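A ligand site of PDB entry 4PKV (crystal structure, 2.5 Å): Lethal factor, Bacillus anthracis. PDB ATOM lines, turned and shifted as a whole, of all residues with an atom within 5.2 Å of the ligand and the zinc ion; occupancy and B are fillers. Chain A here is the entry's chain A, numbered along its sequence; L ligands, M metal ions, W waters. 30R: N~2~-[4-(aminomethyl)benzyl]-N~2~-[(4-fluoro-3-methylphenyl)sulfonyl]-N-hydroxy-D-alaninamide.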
ATOM      1  N   ASP A  64      -5.685  15.340  -5.649  1.00  0.00           N
ATOM      2  CA  ASP A  64      -6.349  14.722  -4.495  1.00  0.00           C
ATOM      3  C   ASP A  64      -7.660  15.427  -4.161  1.00  0.00           C
ATOM      4  O   ASP A  64      -8.357  15.055  -3.220  1.00  0.00           O
ATOM      5  CB  ASP A  64      -5.421  14.701  -3.285  1.00  0.00           C
ATOM      6  CG  ASP A  64      -4.189  13.819  -3.506  1.00  0.00           C
ATOM      7  OD1 ASP A  64      -4.344  12.590  -3.729  1.00  0.00           O
ATOM      8  OD2 ASP A  64      -3.056  14.360  -3.451  1.00  0.00           O
ATOM      9  N   SER A  66     -10.088  15.283  -6.181  1.00  0.00           N
ATOM     10  CA  SER A  66     -11.069  14.413  -6.867  1.00  0.00           C
ATOM     11  C   SER A  66     -11.871  13.601  -5.888  1.00  0.00           C
ATOM     12  O   SER A  66     -11.352  13.157  -4.855  1.00  0.00           O
ATOM     13  CB  SER A  66     -10.390  13.438  -7.820  1.00  0.00           C
ATOM     14  OG  SER A  66      -9.255  13.998  -8.424  1.00  0.00           O
ATOM     15  N   ASP A  67     -13.133  13.360  -6.219  1.00  0.00           N
ATOM     16  CA  ASP A  67     -13.969  12.533  -5.384  1.00  0.00           C
ATOM     17  C   ASP A  67     -14.514  11.311  -6.125  1.00  0.00           C
ATOM     18  O   ASP A  67     -15.600  10.825  -5.802  1.00  0.00           O
ATOM     19  CB  ASP A  67     -15.124  13.368  -4.803  1.00  0.00           C
ATOM     20  CG  ASP A  67     -15.879  14.167  -5.870  1.00  0.00           C
ATOM     21  OD1 ASP A  67     -15.626  13.943  -7.085  1.00  0.00           O
ATOM     22  OD2 ASP A  67     -16.748  14.977  -5.496  1.00  0.00           O
ATOM     23  N   PHE A  68     -13.767  10.804  -7.111  1.00  0.00           N
ATOM     24  CA  PHE A  68     -14.255   9.681  -7.904  1.00  0.00           C
ATOM     25  C   PHE A  68     -13.175   8.736  -8.421  1.00  0.00           C
ATOM     26  O   PHE A  68     -13.480   7.602  -8.789  1.00  0.00           O
ATOM     27  CB  PHE A  68     -15.091  10.200  -9.085  1.00  0.00           C
ATOM     28  CG  PHE A  68     -14.369  11.195  -9.932  1.00  0.00           C
ATOM     29  CD1 PHE A  68     -13.522  10.784 -10.958  1.00  0.00           C
ATOM     30  CD2 PHE A  68     -14.549  12.566  -9.715  1.00  0.00           C
ATOM     31  CE1 PHE A  68     -12.846  11.718 -11.749  1.00  0.00           C
ATOM     32  CE2 PHE A  68     -13.895  13.502 -10.495  1.00  0.00           C
ATOM     33  CZ  PHE A  68     -13.036  13.080 -11.515  1.00  0.00           C
ATOM     34  N   VAL A 392     -18.078   5.934 -10.325  1.00  0.00           N
ATOM     35  CA  VAL A 392     -17.341   6.483  -9.176  1.00  0.00           C
ATOM     36  C   VAL A 392     -16.679   5.412  -8.316  1.00  0.00           C
ATOM     37  O   VAL A 392     -17.318   4.434  -7.957  1.00  0.00           O
ATOM     38  CB  VAL A 392     -18.318   7.345  -8.288  1.00  0.00           C
ATOM     39  CG1 VAL A 392     -17.605   7.934  -7.066  1.00  0.00           C
ATOM     40  CG2 VAL A 392     -18.961   8.450  -9.116  1.00  0.00           C
ATOM     41  N   SER A 394     -15.333   5.163  -4.555  1.00  0.00           N
ATOM     42  CA  SER A 394     -15.286   5.894  -3.292  1.00  0.00           C
ATOM     43  C   SER A 394     -15.581   4.945  -2.143  1.00  0.00           C
ATOM     44  O   SER A 394     -15.873   3.776  -2.371  1.00  0.00           O
ATOM     45  CB  SER A 394     -16.274   7.092  -3.262  1.00  0.00           C
ATOM     46  OG  SER A 394     -17.644   6.675  -3.296  1.00  0.00           O
ATOM     47  N   LYS A 395     -15.523   5.458  -0.917  1.00  0.00           N
ATOM     48  CA  LYS A 395     -15.856   4.683   0.272  1.00  0.00           C
ATOM     49  C   LYS A 395     -17.353   4.361   0.294  1.00  0.00           C
ATOM     50  O   LYS A 395     -17.771   3.304   0.763  1.00  0.00           O
ATOM     51  CB  LYS A 395     -15.464   5.464   1.538  1.00  0.00           C
ATOM     52  CG  LYS A 395     -15.833   4.817   2.855  1.00  0.00           C
ATOM     53  CD  LYS A 395     -14.823   3.741   3.212  1.00  0.00           C
ATOM     54  CE  LYS A 395     -15.096   3.096   4.551  1.00  0.00           C
ATOM     55  NZ  LYS A 395     -14.124   1.992   4.794  1.00  0.00           N
ATOM     56  N   GLY A 396     -18.155   5.294  -0.199  1.00  0.00           N
ATOM     57  CA  GLY A 396     -19.592   5.179  -0.077  1.00  0.00           C
ATOM     58  C   GLY A 396     -20.322   5.940  -1.166  1.00  0.00           C
ATOM     59  O   GLY A 396     -19.840   6.938  -1.685  1.00  0.00           O
ATOM     60  N   LEU A 397     -21.496   5.443  -1.523  1.00  0.00           N
ATOM     61  CA  LEU A 397     -22.271   6.018  -2.597  1.00  0.00           C
ATOM     62  C   LEU A 397     -23.756   5.810  -2.313  1.00  0.00           C
ATOM     63  O   LEU A 397     -24.156   4.790  -1.777  1.00  0.00           O
ATOM     64  CB  LEU A 397     -21.872   5.381  -3.929  1.00  0.00           C
ATOM     65  CG  LEU A 397     -22.160   6.172  -5.218  1.00  0.00           C
ATOM     66  CD1 LEU A 397     -21.268   7.386  -5.244  1.00  0.00           C
ATOM     67  CD2 LEU A 397     -21.980   5.337  -6.480  1.00  0.00           C
ATOM     68  N   TYR A 398     -24.587   6.793  -2.658  1.00  0.00           N
ATOM     69  CA  TYR A 398     -26.010   6.527  -2.767  1.00  0.00           C
ATOM     70  C   TYR A 398     -26.418   6.646  -4.244  1.00  0.00           C
ATOM     71  O   TYR A 398     -26.121   7.644  -4.893  1.00  0.00           O
ATOM     72  CB  TYR A 398     -26.839   7.469  -1.890  1.00  0.00           C
ATOM     73  CG  TYR A 398     -28.335   7.335  -2.107  1.00  0.00           C
ATOM     74  CD1 TYR A 398     -29.012   6.197  -1.682  1.00  0.00           C
ATOM     75  CD2 TYR A 398     -29.070   8.323  -2.737  1.00  0.00           C
ATOM     76  CE1 TYR A 398     -30.359   6.042  -1.889  1.00  0.00           C
ATOM     77  CE2 TYR A 398     -30.442   8.184  -2.932  1.00  0.00           C
ATOM     78  CZ  TYR A 398     -31.068   7.044  -2.509  1.00  0.00           C
ATOM     79  OH  TYR A 398     -32.416   6.889  -2.698  1.00  0.00           O
ATOM     80  N   GLY A 413     -12.046   6.613   4.070  1.00  0.00           N
ATOM     81  CA  GLY A 413     -12.613   7.877   3.628  1.00  0.00           C
ATOM     82  C   GLY A 413     -11.874   9.061   4.211  1.00  0.00           C
ATOM     83  O   GLY A 413     -11.543   9.087   5.401  1.00  0.00           O
ATOM     84  N   VAL A 414     -11.584  10.035   3.367  1.00  0.00           N
ATOM     85  CA  VAL A 414     -11.020  11.302   3.812  1.00  0.00           C
ATOM     86  C   VAL A 414     -11.954  11.952   4.812  1.00  0.00           C
ATOM     87  O   VAL A 414     -13.168  11.903   4.605  1.00  0.00           O
ATOM     88  CB  VAL A 414     -10.801  12.245   2.612  1.00  0.00           C
ATOM     89  CG1 VAL A 414     -10.459  13.661   3.084  1.00  0.00           C
ATOM     90  CG2 VAL A 414      -9.723  11.661   1.665  1.00  0.00           C
ATOM     91  N   GLU A 415     -11.431  12.526   5.900  1.00  0.00           N
ATOM     92  CA  GLU A 415     -12.278  13.325   6.788  1.00  0.00           C
ATOM     93  C   GLU A 415     -13.264  12.438   7.595  1.00  0.00           C
ATOM     94  O   GLU A 415     -14.167  12.917   8.278  1.00  0.00           O
ATOM     95  CB  GLU A 415     -13.004  14.402   5.929  1.00  0.00           C
ATOM     96  CG  GLU A 415     -14.164  15.221   6.521  1.00  0.00           C
ATOM     97  CD  GLU A 415     -13.704  16.425   7.341  1.00  0.00           C
ATOM     98  OE1 GLU A 415     -12.692  17.065   6.955  1.00  0.00           O
ATOM     99  OE2 GLU A 415     -14.348  16.726   8.368  1.00  0.00           O
ATOM    100  N   LEU A 416     -13.076  11.119   7.526  1.00  0.00           N
ATOM    101  CA  LEU A 416     -13.975  10.199   8.240  1.00  0.00           C
ATOM    102  C   LEU A 416     -13.296   9.517   9.425  1.00  0.00           C
ATOM    103  O   LEU A 416     -12.137   9.096   9.341  1.00  0.00           O
ATOM    104  CB  LEU A 416     -14.518   9.144   7.283  1.00  0.00           C
ATOM    105  CG  LEU A 416     -15.640   9.586   6.348  1.00  0.00           C
ATOM    106  CD1 LEU A 416     -16.176   8.371   5.553  1.00  0.00           C
ATOM    107  CD2 LEU A 416     -16.763  10.298   7.129  1.00  0.00           C
ATOM    108  N   GLY A 422     -19.482   7.297   7.483  1.00  0.00           N
ATOM    109  CA  GLY A 422     -19.675   7.216   6.045  1.00  0.00           C
ATOM    110  C   GLY A 422     -21.067   6.751   5.685  1.00  0.00           C
ATOM    111  O   GLY A 422     -21.708   7.330   4.793  1.00  0.00           O
ATOM    112  N   HIS A 425     -23.826   9.489   6.236  1.00  0.00           N
ATOM    113  CA  HIS A 425     -23.803  10.512   5.198  1.00  0.00           C
ATOM    114  C   HIS A 425     -24.562   9.991   3.962  1.00  0.00           C
ATOM    115  O   HIS A 425     -25.348  10.726   3.343  1.00  0.00           O
ATOM    116  CB  HIS A 425     -22.351  10.886   4.896  1.00  0.00           C
ATOM    117  CG  HIS A 425     -22.120  11.513   3.553  1.00  0.00           C
ATOM    118  ND1 HIS A 425     -21.671  12.801   3.398  1.00  0.00           N
ATOM    119  CD2 HIS A 425     -22.210  10.990   2.306  1.00  0.00           C
ATOM    120  CE1 HIS A 425     -21.527  13.072   2.107  1.00  0.00           C
ATOM    121  NE2 HIS A 425     -21.854  11.994   1.425  1.00  0.00           N
ATOM    122  N   GLU A 426     -24.361   8.722   3.619  1.00  0.00           N
ATOM    123  CA  GLU A 426     -25.116   8.134   2.530  1.00  0.00           C
ATOM    124  C   GLU A 426     -26.591   8.092   2.859  1.00  0.00           C
ATOM    125  O   GLU A 426     -27.435   8.241   1.983  1.00  0.00           O
ATOM    126  CB  GLU A 426     -24.638   6.703   2.213  1.00  0.00           C
ATOM    127  CG  GLU A 426     -23.129   6.557   2.071  1.00  0.00           C
ATOM    128  CD  GLU A 426     -22.550   7.441   0.989  1.00  0.00           C
ATOM    129  OE1 GLU A 426     -21.372   7.828   1.096  1.00  0.00           O
ATOM    130  OE2 GLU A 426     -23.288   7.759   0.017  1.00  0.00           O
ATOM    131  N   HIS A 429     -28.090  11.245   1.855  1.00  0.00           N
ATOM    132  CA  HIS A 429     -28.579  11.362   0.477  1.00  0.00           C
ATOM    133  C   HIS A 429     -29.963  10.745   0.274  1.00  0.00           C
ATOM    134  O   HIS A 429     -30.780  11.271  -0.468  1.00  0.00           O
ATOM    135  CB  HIS A 429     -27.632  10.708  -0.506  1.00  0.00           C
ATOM    136  CG  HIS A 429     -26.344  11.432  -0.675  1.00  0.00           C
ATOM    137  ND1 HIS A 429     -26.286  12.769  -1.004  1.00  0.00           N
ATOM    138  CD2 HIS A 429     -25.064  10.996  -0.621  1.00  0.00           C
ATOM    139  CE1 HIS A 429     -25.021  13.132  -1.123  1.00  0.00           C
ATOM    140  NE2 HIS A 429     -24.263  12.076  -0.895  1.00  0.00           N
ATOM    141  N   TYR A 467     -15.396  19.346   2.270  1.00  0.00           N
ATOM    142  CA  TYR A 467     -16.110  18.616   1.215  1.00  0.00           C
ATOM    143  C   TYR A 467     -17.582  19.081   1.048  1.00  0.00           C
ATOM    144  O   TYR A 467     -18.197  18.879  -0.019  1.00  0.00           O
ATOM    145  CB  TYR A 467     -16.056  17.109   1.487  1.00  0.00           C
ATOM    146  CG  TYR A 467     -16.731  16.286   0.412  1.00  0.00           C
ATOM    147  CD1 TYR A 467     -16.284  16.304  -0.908  1.00  0.00           C
ATOM    148  CD2 TYR A 467     -17.836  15.503   0.719  1.00  0.00           C
ATOM    149  CE1 TYR A 467     -16.922  15.560  -1.889  1.00  0.00           C
ATOM    150  CE2 TYR A 467     -18.476  14.752  -0.255  1.00  0.00           C
ATOM    151  CZ  TYR A 467     -18.019  14.780  -1.559  1.00  0.00           C
ATOM    152  OH  TYR A 467     -18.685  14.016  -2.509  1.00  0.00           O
ATOM    153  N   GLU A 474     -24.041  17.433  -1.502  1.00  0.00           N
ATOM    154  CA  GLU A 474     -22.987  17.061  -0.568  1.00  0.00           C
ATOM    155  C   GLU A 474     -23.079  17.897   0.710  1.00  0.00           C
ATOM    156  O   GLU A 474     -22.879  17.369   1.821  1.00  0.00           O
ATOM    157  CB  GLU A 474     -21.608  17.214  -1.218  1.00  0.00           C
ATOM    158  CG  GLU A 474     -21.397  16.358  -2.480  1.00  0.00           C
ATOM    159  CD  GLU A 474     -21.842  14.904  -2.300  1.00  0.00           C
ATOM    160  OE1 GLU A 474     -21.749  14.386  -1.182  1.00  0.00           O
ATOM    161  OE2 GLU A 474     -22.283  14.282  -3.289  1.00  0.00           O
ATOM    162  N   ALA A 477     -25.660  16.449   2.839  1.00  0.00           N
ATOM    163  CA  ALA A 477     -25.274  15.143   3.345  1.00  0.00           C
ATOM    164  C   ALA A 477     -24.307  15.262   4.513  1.00  0.00           C
ATOM    165  O   ALA A 477     -24.444  14.557   5.499  1.00  0.00           O
ATOM    166  CB  ALA A 477     -24.658  14.284   2.220  1.00  0.00           C
ATOM    167  N   GLU A 478     -23.338  16.155   4.377  1.00  0.00           N
ATOM    168  CA  GLU A 478     -22.390  16.412   5.465  1.00  0.00           C
ATOM    169  C   GLU A 478     -23.108  16.966   6.714  1.00  0.00           C
ATOM    170  O   GLU A 478     -22.955  16.427   7.827  1.00  0.00           O
ATOM    171  CB  GLU A 478     -21.286  17.348   4.973  1.00  0.00           C
ATOM    172  CG  GLU A 478     -20.272  16.669   4.030  1.00  0.00           C
ATOM    173  CD  GLU A 478     -19.375  15.629   4.735  1.00  0.00           C
ATOM    174  OE1 GLU A 478     -18.157  15.896   4.904  1.00  0.00           O
ATOM    175  OE2 GLU A 478     -19.886  14.530   5.102  1.00  0.00           O
ATOM    176  N   ARG A 481     -24.760  14.452   8.451  1.00  0.00           N
ATOM    177  CA  ARG A 481     -23.848  13.540   9.139  1.00  0.00           C
ATOM    178  C   ARG A 481     -23.410  14.145  10.463  1.00  0.00           C
ATOM    179  O   ARG A 481     -23.450  13.474  11.492  1.00  0.00           O
ATOM    180  CB  ARG A 481     -22.613  13.218   8.292  1.00  0.00           C
ATOM    181  CG  ARG A 481     -21.602  12.369   9.045  1.00  0.00           C
ATOM    182  CD  ARG A 481     -20.425  11.975   8.185  1.00  0.00           C
ATOM    183  NE  ARG A 481     -19.631  13.112   7.753  1.00  0.00           N
ATOM    184  CZ  ARG A 481     -18.706  13.708   8.503  1.00  0.00           C
ATOM    185  NH1 ARG A 481     -18.474  13.288   9.743  1.00  0.00           N
ATOM    186  NH2 ARG A 481     -18.032  14.733   8.003  1.00  0.00           N
HETATM  187  C1  30R L   1     -18.321   9.832  -1.938  1.00  0.00           C
HETATM  188  C2  30R L   1     -19.691  10.408  -1.575  1.00  0.00           C
HETATM  189  C3  30R L   1     -11.229  13.489  -0.964  1.00  0.00           C
HETATM  190  O3  30R L   1     -20.057  11.827  -1.559  1.00  0.00           O
HETATM  191  N4  30R L   1     -20.700   9.576  -1.261  1.00  0.00           N
HETATM  192  N5  30R L   1     -11.275  14.672  -0.054  1.00  0.00           N
HETATM  193  C10 30R L   1     -16.992   9.965   1.443  1.00  0.00           C
HETATM  194  C11 30R L   1     -16.278  11.060   1.938  1.00  0.00           C
HETATM  195  C12 30R L   1     -16.684  11.703   3.097  1.00  0.00           C
HETATM  196  C13 30R L   1     -17.822  11.261   3.749  1.00  0.00           C
HETATM  197  C14 30R L   1     -18.560  10.182   3.264  1.00  0.00           C
HETATM  198  C15 30R L   1     -18.151   9.526   2.106  1.00  0.00           C
HETATM  199  C17 30R L   1     -15.909  12.880   3.635  1.00  0.00           C
HETATM  200  C18 30R L   1     -16.697  11.512  -1.443  1.00  0.00           C
HETATM  201  C19 30R L   1     -15.246  11.951  -1.354  1.00  0.00           C
HETATM  202  C20 30R L   1     -14.219  11.391  -2.129  1.00  0.00           C
HETATM  203  C21 30R L   1     -12.916  11.883  -1.993  1.00  0.00           C
HETATM  204  C22 30R L   1     -12.639  12.934  -1.118  1.00  0.00           C
HETATM  205  C23 30R L   1     -13.670  13.507  -0.362  1.00  0.00           C
HETATM  206  C24 30R L   1     -14.955  13.027  -0.492  1.00  0.00           C
HETATM  207  C28 30R L   1     -18.078  10.246  -3.394  1.00  0.00           C
HETATM  208  N6  30R L   1     -17.133  10.162  -1.083  1.00  0.00           N
HETATM  209  O5  30R L   1     -21.943  10.061  -1.046  1.00  0.00           O
HETATM  210  S7  30R L   1     -16.515   9.267   0.077  1.00  0.00           S
HETATM  211  O8  30R L   1     -15.055   9.152   0.120  1.00  0.00           O
HETATM  212  O9  30R L   1     -17.002   7.902   0.010  1.00  0.00           O
HETATM  213  F16 30R L   1     -18.203  11.887   4.879  1.00  0.00           F
HETATM  214 ZN    ZN M   1     -22.032  12.136  -0.954  1.00  0.00          ZN
HETATM  215  O   HOH W   1     -23.639   9.626  -3.252  1.00  0.00           O
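An oxygen (O3) of the ligand lies close to the side-chain hydroxyl (OH) of Tyr 467, at 2.8 Å. The backbone NH (N) of Gly 396 lies within hydrogen-bond range of an oxygen (O9) of the ligand. The backbone carbonyl oxygen of Gly 396 lies within hydrogen-bond range of a nitrogen (N4) of the ligand (2.8 Å). N4 of the ligand lies within hydrogen-bond range of OE1 of Glu 426, at 3.0 Å. The backbone NH (N) of Lys 395 lies within hydrogen-bond range of an oxygen (O9) of the ligand.
The side-chain hydroxyl of Tyr 467 lies close to the side-chain carboxylate of Glu 474, 3.4 Å away. OE2 of Glu 478 is in hydrogen-bond range of ND1 of His 425. The backbone carbonyl oxygen of Gly 396 lies within hydrogen-bond range of the side-chain hydroxyl of Ser 394 (2.7 Å). OE2 of Glu 426 lies close to N of Leu 397, at 3.3 Å. N of Tyr 398 lies within hydrogen-bond range of OE2 of Glu 426 (3.1 Å). The side-chain carboxylate of Glu 478 lies within salt-bridge range of the guanidinium group of Arg 481.
The side-chain carboxylate (OE2) of Glu 478 sits close to a fluorine (F16) of the ligand (3.1 Å). A fluorine (F16) of the ligand lies close to the guanidinium group of Arg 481, at 3.4 Å. O of Asp 64 touches C3 of the ligand (3.97 Å). O of Ser 66 touches C21 of the ligand (3.5 Å). Asp 67 touches the ligand. CB of Ser 394 touches O9 of the ligand (3.4 Å). Val 414 touches the ligand. CD2 of Leu 416 touches F16 of the ligand (3.1 Å). Hydrophobic or aromatic side chains within 4 Å of the ligand: Val 414, Leu 416, His 425, His 429 and Tyr 467.
Of the 23 residues printed, 3 come within 4 Å of the zinc ion. The nearest printed residue that does not touch the zinc ion is Tyr 467 (4.1 Å).
The zinc ion is bound by an oxygen (O5) of the ligand (2.1 Å), an oxygen (O3) of the ligand (2.1 Å), a ring nitrogen (NE2) of His 429 (2.2 Å), the side-chain carboxylate (OE1) of Glu 474 (2.3 Å) and a ring nitrogen (NE2) of His 425 (2.4 Å).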
